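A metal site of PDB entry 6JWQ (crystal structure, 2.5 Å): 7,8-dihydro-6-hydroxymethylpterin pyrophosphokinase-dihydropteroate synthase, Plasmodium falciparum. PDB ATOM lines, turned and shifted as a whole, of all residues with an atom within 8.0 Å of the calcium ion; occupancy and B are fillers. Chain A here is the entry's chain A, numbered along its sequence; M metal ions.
The calcium ion is bound by the backbone carbonyl oxygen (O) of Glu 42 (2.5 Å), the side-chain carboxylate (OE1) of Glu 42 (2.5 Å), the side-chain carboxylate (OE1) of Glu 99 (2.6 Å), the backbone carbonyl oxygen (O) of Gly 46 (2.8 Å) and the side-chain carboxylate (OE2) of Glu 99 (2.9 Å).
The side-chain carboxylate of Glu 42 lies within hydrogen-bond range of the backbone NH of Ile 48 (3.0 Å).
Of the 21 residues printed, 3 come within 4 Å of the calcium ion.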
ATOM      1  N   LEU A  38       6.193 -28.300  34.348  1.00  0.00           N
ATOM      2  CA  LEU A  38       5.315 -27.195  34.765  1.00  0.00           C
ATOM      3  C   LEU A  38       5.312 -26.022  33.777  1.00  0.00           C
ATOM      4  O   LEU A  38       4.230 -25.489  33.459  1.00  0.00           O
ATOM      5  CB  LEU A  38       5.692 -26.666  36.150  1.00  0.00           C
ATOM      6  CG  LEU A  38       5.258 -27.363  37.429  1.00  0.00           C
ATOM      7  CD1 LEU A  38       5.717 -26.581  38.627  1.00  0.00           C
ATOM      8  CD2 LEU A  38       3.761 -27.502  37.484  1.00  0.00           C
ATOM      9  N   HIS A  39       6.501 -25.619  33.316  1.00  0.00           N
ATOM     10  CA  HIS A  39       6.576 -24.443  32.444  1.00  0.00           C
ATOM     11  C   HIS A  39       5.982 -24.700  31.071  1.00  0.00           C
ATOM     12  O   HIS A  39       5.253 -23.850  30.561  1.00  0.00           O
ATOM     13  CB  HIS A  39       7.985 -23.825  32.305  1.00  0.00           C
ATOM     14  CG  HIS A  39       8.026 -22.712  31.293  1.00  0.00           C
ATOM     15  ND1 HIS A  39       7.375 -21.502  31.487  1.00  0.00           N
ATOM     16  CD2 HIS A  39       8.580 -22.640  30.054  1.00  0.00           C
ATOM     17  CE1 HIS A  39       7.552 -20.738  30.423  1.00  0.00           C
ATOM     18  NE2 HIS A  39       8.284 -21.400  29.542  1.00  0.00           N
ATOM     19  N   LEU A  40       6.284 -25.858  30.494  1.00  0.00           N
ATOM     20  CA  LEU A  40       5.691 -26.272  29.224  1.00  0.00           C
ATOM     21  C   LEU A  40       4.166 -26.347  29.349  1.00  0.00           C
ATOM     22  O   LEU A  40       3.468 -25.866  28.465  1.00  0.00           O
ATOM     23  CB  LEU A  40       6.300 -27.581  28.706  1.00  0.00           C
ATOM     24  CG  LEU A  40       7.814 -27.518  28.399  1.00  0.00           C
ATOM     25  CD1 LEU A  40       8.441 -28.898  28.305  1.00  0.00           C
ATOM     26  CD2 LEU A  40       8.132 -26.708  27.152  1.00  0.00           C
ATOM     27  N   VAL A  41       3.667 -26.865  30.481  1.00  0.00           N
ATOM     28  CA  VAL A  41       2.214 -26.824  30.771  1.00  0.00           C
ATOM     29  C   VAL A  41       1.672 -25.390  30.762  1.00  0.00           C
ATOM     30  O   VAL A  41       0.653 -25.163  30.102  1.00  0.00           O
ATOM     31  CB  VAL A  41       1.795 -27.594  32.056  1.00  0.00           C
ATOM     32  CG1 VAL A  41       0.324 -27.370  32.381  1.00  0.00           C
ATOM     33  CG2 VAL A  41       2.055 -29.089  31.927  1.00  0.00           C
ATOM     34  N   GLU A  42       2.335 -24.449  31.445  1.00  0.00           N
ATOM     35  CA  GLU A  42       1.942 -23.013  31.386  1.00  0.00           C
ATOM     36  C   GLU A  42       2.014 -22.445  29.980  1.00  0.00           C
ATOM     37  O   GLU A  42       1.237 -21.528  29.619  1.00  0.00           O
ATOM     38  CB  GLU A  42       2.803 -22.122  32.263  1.00  0.00           C
ATOM     39  CG  GLU A  42       2.244 -21.786  33.634  1.00  0.00           C
ATOM     40  CD  GLU A  42       1.132 -20.725  33.672  1.00  0.00           C
ATOM     41  OE1 GLU A  42       0.792 -20.117  32.613  1.00  0.00           O
ATOM     42  OE2 GLU A  42       0.605 -20.493  34.792  1.00  0.00           O
ATOM     43  N   LYS A  43       2.969 -22.968  29.208  1.00  0.00           N
ATOM     44  CA  LYS A  43       3.237 -22.467  27.872  1.00  0.00           C
ATOM     45  C   LYS A  43       2.200 -23.018  26.931  1.00  0.00           C
ATOM     46  O   LYS A  43       1.612 -22.267  26.174  1.00  0.00           O
ATOM     47  CB  LYS A  43       4.665 -22.827  27.416  1.00  0.00           C
ATOM     48  CG  LYS A  43       5.072 -22.224  26.083  1.00  0.00           C
ATOM     49  CD  LYS A  43       6.570 -22.382  25.830  1.00  0.00           C
ATOM     50  CE  LYS A  43       6.989 -21.778  24.489  1.00  0.00           C
ATOM     51  NZ  LYS A  43       6.659 -20.332  24.303  1.00  0.00           N
ATOM     52  N   TYR A  44       1.968 -24.333  27.011  1.00  0.00           N
ATOM     53  CA  TYR A  44       1.231 -25.045  26.002  1.00  0.00           C
ATOM     54  C   TYR A  44      -0.232 -25.394  26.334  1.00  0.00           C
ATOM     55  O   TYR A  44      -0.976 -25.705  25.414  1.00  0.00           O
ATOM     56  CB  TYR A  44       2.009 -26.280  25.557  1.00  0.00           C
ATOM     57  CG  TYR A  44       3.296 -26.012  24.785  1.00  0.00           C
ATOM     58  CD1 TYR A  44       3.408 -24.950  23.882  1.00  0.00           C
ATOM     59  CD2 TYR A  44       4.394 -26.857  24.935  1.00  0.00           C
ATOM     60  CE1 TYR A  44       4.570 -24.731  23.159  1.00  0.00           C
ATOM     61  CE2 TYR A  44       5.573 -26.656  24.232  1.00  0.00           C
ATOM     62  CZ  TYR A  44       5.659 -25.589  23.342  1.00  0.00           C
ATOM     63  OH  TYR A  44       6.843 -25.397  22.644  1.00  0.00           O
ATOM     64  N   LEU A  45      -0.631 -25.333  27.604  1.00  0.00           N
ATOM     65  CA  LEU A  45      -1.985 -25.800  28.011  1.00  0.00           C
ATOM     66  C   LEU A  45      -2.933 -24.742  28.586  1.00  0.00           C
ATOM     67  O   LEU A  45      -4.137 -24.875  28.476  1.00  0.00           O
ATOM     68  CB  LEU A  45      -1.910 -27.015  28.933  1.00  0.00           C
ATOM     69  CG  LEU A  45      -1.224 -28.262  28.339  1.00  0.00           C
ATOM     70  CD1 LEU A  45      -1.021 -29.390  29.353  1.00  0.00           C
ATOM     71  CD2 LEU A  45      -1.936 -28.755  27.096  1.00  0.00           C
ATOM     72  N   GLY A  46      -2.389 -23.679  29.158  1.00  0.00           N
ATOM     73  CA  GLY A  46      -3.203 -22.685  29.852  1.00  0.00           C
ATOM     74  C   GLY A  46      -2.490 -22.217  31.092  1.00  0.00           C
ATOM     75  O   GLY A  46      -1.262 -22.233  31.158  1.00  0.00           O
ATOM     76  N   LYS A  47      -3.280 -21.818  32.084  1.00  0.00           N
ATOM     77  CA  LYS A  47      -2.762 -21.225  33.300  1.00  0.00           C
ATOM     78  C   LYS A  47      -2.830 -22.182  34.484  1.00  0.00           C
ATOM     79  O   LYS A  47      -3.892 -22.723  34.815  1.00  0.00           O
ATOM     80  CB  LYS A  47      -3.576 -19.959  33.608  1.00  0.00           C
ATOM     81  CG  LYS A  47      -3.150 -19.263  34.889  1.00  0.00           C
ATOM     82  CD  LYS A  47      -3.864 -17.947  35.067  1.00  0.00           C
ATOM     83  CE  LYS A  47      -3.315 -17.217  36.292  1.00  0.00           C
ATOM     84  NZ  LYS A  47      -1.879 -16.843  36.107  1.00  0.00           N
ATOM     85  N   ILE A  48      -1.692 -22.378  35.142  1.00  0.00           N
ATOM     86  CA  ILE A  48      -1.618 -23.101  36.418  1.00  0.00           C
ATOM     87  C   ILE A  48      -2.275 -22.251  37.519  1.00  0.00           C
ATOM     88  O   ILE A  48      -1.843 -21.127  37.774  1.00  0.00           O
ATOM     89  CB  ILE A  48      -0.145 -23.417  36.789  1.00  0.00           C
ATOM     90  CG1 ILE A  48       0.493 -24.270  35.674  1.00  0.00           C
ATOM     91  CG2 ILE A  48      -0.066 -24.076  38.154  1.00  0.00           C
ATOM     92  CD1 ILE A  48       1.794 -24.959  36.052  1.00  0.00           C
ATOM     93  N   SER A  95       3.660 -20.873  21.360  1.00  0.00           N
ATOM     94  CA  SER A  95       2.257 -21.250  21.447  1.00  0.00           C
ATOM     95  C   SER A  95       1.442 -20.261  20.635  1.00  0.00           C
ATOM     96  O   SER A  95       1.757 -19.075  20.605  1.00  0.00           O
ATOM     97  CB  SER A  95       1.811 -21.245  22.916  1.00  0.00           C
ATOM     98  OG  SER A  95       0.399 -21.122  23.050  1.00  0.00           O
ATOM     99  N   TYR A  97      -1.460 -19.656  21.581  1.00  0.00           N
ATOM    100  CA  TYR A  97      -2.273 -19.043  22.629  1.00  0.00           C
ATOM    101  C   TYR A  97      -1.412 -18.161  23.541  1.00  0.00           C
ATOM    102  O   TYR A  97      -0.190 -18.352  23.649  1.00  0.00           O
ATOM    103  CB  TYR A  97      -3.021 -20.099  23.435  1.00  0.00           C
ATOM    104  CG  TYR A  97      -4.290 -20.604  22.799  1.00  0.00           C
ATOM    105  CD1 TYR A  97      -4.266 -21.577  21.793  1.00  0.00           C
ATOM    106  CD2 TYR A  97      -5.536 -20.107  23.215  1.00  0.00           C
ATOM    107  CE1 TYR A  97      -5.452 -22.034  21.206  1.00  0.00           C
ATOM    108  CE2 TYR A  97      -6.715 -20.557  22.638  1.00  0.00           C
ATOM    109  CZ  TYR A  97      -6.663 -21.522  21.647  1.00  0.00           C
ATOM    110  OH  TYR A  97      -7.825 -21.984  21.078  1.00  0.00           O
ATOM    111  N   GLU A  98      -2.065 -17.210  24.181  1.00  0.00           N
ATOM    112  CA  GLU A  98      -1.342 -16.143  24.873  1.00  0.00           C
ATOM    113  C   GLU A  98      -1.121 -16.373  26.366  1.00  0.00           C
ATOM    114  O   GLU A  98      -1.910 -17.050  27.024  1.00  0.00           O
ATOM    115  CB  GLU A  98      -2.002 -14.790  24.633  1.00  0.00           C
ATOM    116  CG  GLU A  98      -3.507 -14.790  24.857  1.00  0.00           C
ATOM    117  CD  GLU A  98      -4.088 -13.401  24.895  1.00  0.00           C
ATOM    118  OE1 GLU A  98      -3.596 -12.520  24.154  1.00  0.00           O
ATOM    119  OE2 GLU A  98      -5.042 -13.216  25.675  1.00  0.00           O
ATOM    120  N   GLU A  99      -0.038 -15.782  26.854  1.00  0.00           N
ATOM    121  CA  GLU A  99       0.334 -15.758  28.253  1.00  0.00           C
ATOM    122  C   GLU A  99      -0.103 -14.461  28.916  1.00  0.00           C
ATOM    123  O   GLU A  99       0.109 -13.375  28.375  1.00  0.00           O
ATOM    124  CB  GLU A  99       1.856 -15.919  28.352  1.00  0.00           C
ATOM    125  CG  GLU A  99       2.366 -16.277  29.732  1.00  0.00           C
ATOM    126  CD  GLU A  99       1.777 -17.567  30.230  1.00  0.00           C
ATOM    127  OE1 GLU A  99       0.760 -17.515  30.960  1.00  0.00           O
ATOM    128  OE2 GLU A  99       2.300 -18.643  29.855  1.00  0.00           O
ATOM    129  N   ASN A 100      -0.743 -14.569  30.080  1.00  0.00           N
ATOM    130  CA  ASN A 100      -1.126 -13.377  30.853  1.00  0.00           C
ATOM    131  C   ASN A 100      -0.657 -13.465  32.301  1.00  0.00           C
ATOM    132  O   ASN A 100      -1.156 -14.274  33.082  1.00  0.00           O
ATOM    133  CB  ASN A 100      -2.625 -13.092  30.797  1.00  0.00           C
ATOM    134  CG  ASN A 100      -3.134 -12.842  29.386  1.00  0.00           C
ATOM    135  OD1 ASN A 100      -4.255 -13.234  29.075  1.00  0.00           O
ATOM    136  ND2 ASN A 100      -2.340 -12.183  28.542  1.00  0.00           N
ATOM    137  N   LYS A 101       0.305 -12.606  32.632  1.00  0.00           N
ATOM    138  CA  LYS A 101       0.918 -12.622  33.953  1.00  0.00           C
ATOM    139  C   LYS A 101       0.208 -11.769  35.007  1.00  0.00           C
ATOM    140  O   LYS A 101       0.611 -11.804  36.153  1.00  0.00           O
ATOM    141  CB  LYS A 101       2.408 -12.258  33.849  1.00  0.00           C
ATOM    142  CG  LYS A 101       3.251 -13.297  33.101  1.00  0.00           C
ATOM    143  CD  LYS A 101       4.734 -12.941  32.987  1.00  0.00           C
ATOM    144  CE  LYS A 101       5.477 -12.908  34.337  1.00  0.00           C
ATOM    145  NZ  LYS A 101       5.632 -14.224  35.073  1.00  0.00           N
ATOM    146  N   VAL A 170      -4.934 -26.831  35.878  1.00  0.00           N
ATOM    147  CA  VAL A 170      -4.771 -25.934  34.726  1.00  0.00           C
ATOM    148  C   VAL A 170      -6.131 -25.424  34.270  1.00  0.00           C
ATOM    149  O   VAL A 170      -7.061 -26.212  34.043  1.00  0.00           O
ATOM    150  CB  VAL A 170      -4.082 -26.606  33.535  1.00  0.00           C
ATOM    151  CG1 VAL A 170      -3.616 -25.576  32.505  1.00  0.00           C
ATOM    152  CG2 VAL A 170      -2.898 -27.459  33.989  1.00  0.00           C
ATOM    153  N   LYS A 171      -6.261 -24.103  34.184  1.00  0.00           N
ATOM    154  CA  LYS A 171      -7.360 -23.481  33.457  1.00  0.00           C
ATOM    155  C   LYS A 171      -6.931 -23.500  31.999  1.00  0.00           C
ATOM    156  O   LYS A 171      -6.061 -22.714  31.565  1.00  0.00           O
ATOM    157  CB  LYS A 171      -7.630 -22.063  33.973  1.00  0.00           C
ATOM    158  CG  LYS A 171      -8.508 -21.204  33.088  1.00  0.00           C
ATOM    159  CD  LYS A 171      -8.266 -19.727  33.349  1.00  0.00           C
ATOM    160  CE  LYS A 171      -9.369 -19.128  34.210  1.00  0.00           C
ATOM    161  NZ  LYS A 171      -8.813 -18.302  35.322  1.00  0.00           N
ATOM    162  N   PHE A 173      -7.119 -23.833  27.705  1.00  0.00           N
ATOM    163  CA  PHE A 173      -7.752 -23.391  26.463  1.00  0.00           C
ATOM    164  C   PHE A 173      -7.923 -24.584  25.486  1.00  0.00           C
ATOM    165  O   PHE A 173      -8.444 -24.433  24.383  1.00  0.00           O
ATOM    166  CB  PHE A 173      -6.978 -22.200  25.836  1.00  0.00           C
ATOM    167  CG  PHE A 173      -5.468 -22.379  25.797  1.00  0.00           C
ATOM    168  CD1 PHE A 173      -4.875 -23.379  24.996  1.00  0.00           C
ATOM    169  CD2 PHE A 173      -4.630 -21.552  26.549  1.00  0.00           C
ATOM    170  CE1 PHE A 173      -3.487 -23.540  24.964  1.00  0.00           C
ATOM    171  CE2 PHE A 173      -3.241 -21.713  26.517  1.00  0.00           C
ATOM    172  CZ  PHE A 173      -2.667 -22.703  25.730  1.00  0.00           C
ATOM    173  N   LYS A 518       8.623 -16.024  38.826  1.00  0.00           N
ATOM    174  CA  LYS A 518       8.735 -16.922  37.678  1.00  0.00           C
ATOM    175  C   LYS A 518       9.528 -16.257  36.573  1.00  0.00           C
ATOM    176  O   LYS A 518       9.180 -15.154  36.156  1.00  0.00           O
ATOM    177  CB  LYS A 518       7.359 -17.299  37.126  1.00  0.00           C
ATOM    178  CG  LYS A 518       6.349 -17.787  38.164  1.00  0.00           C
ATOM    179  CD  LYS A 518       4.984 -17.129  37.919  1.00  0.00           C
ATOM    180  CE  LYS A 518       3.915 -18.186  37.741  1.00  0.00           C
ATOM    181  NZ  LYS A 518       2.594 -17.650  37.329  1.00  0.00           N
HETATM  182 CA    CA M   1      -0.308 -19.765  30.365  1.00  0.00          CA
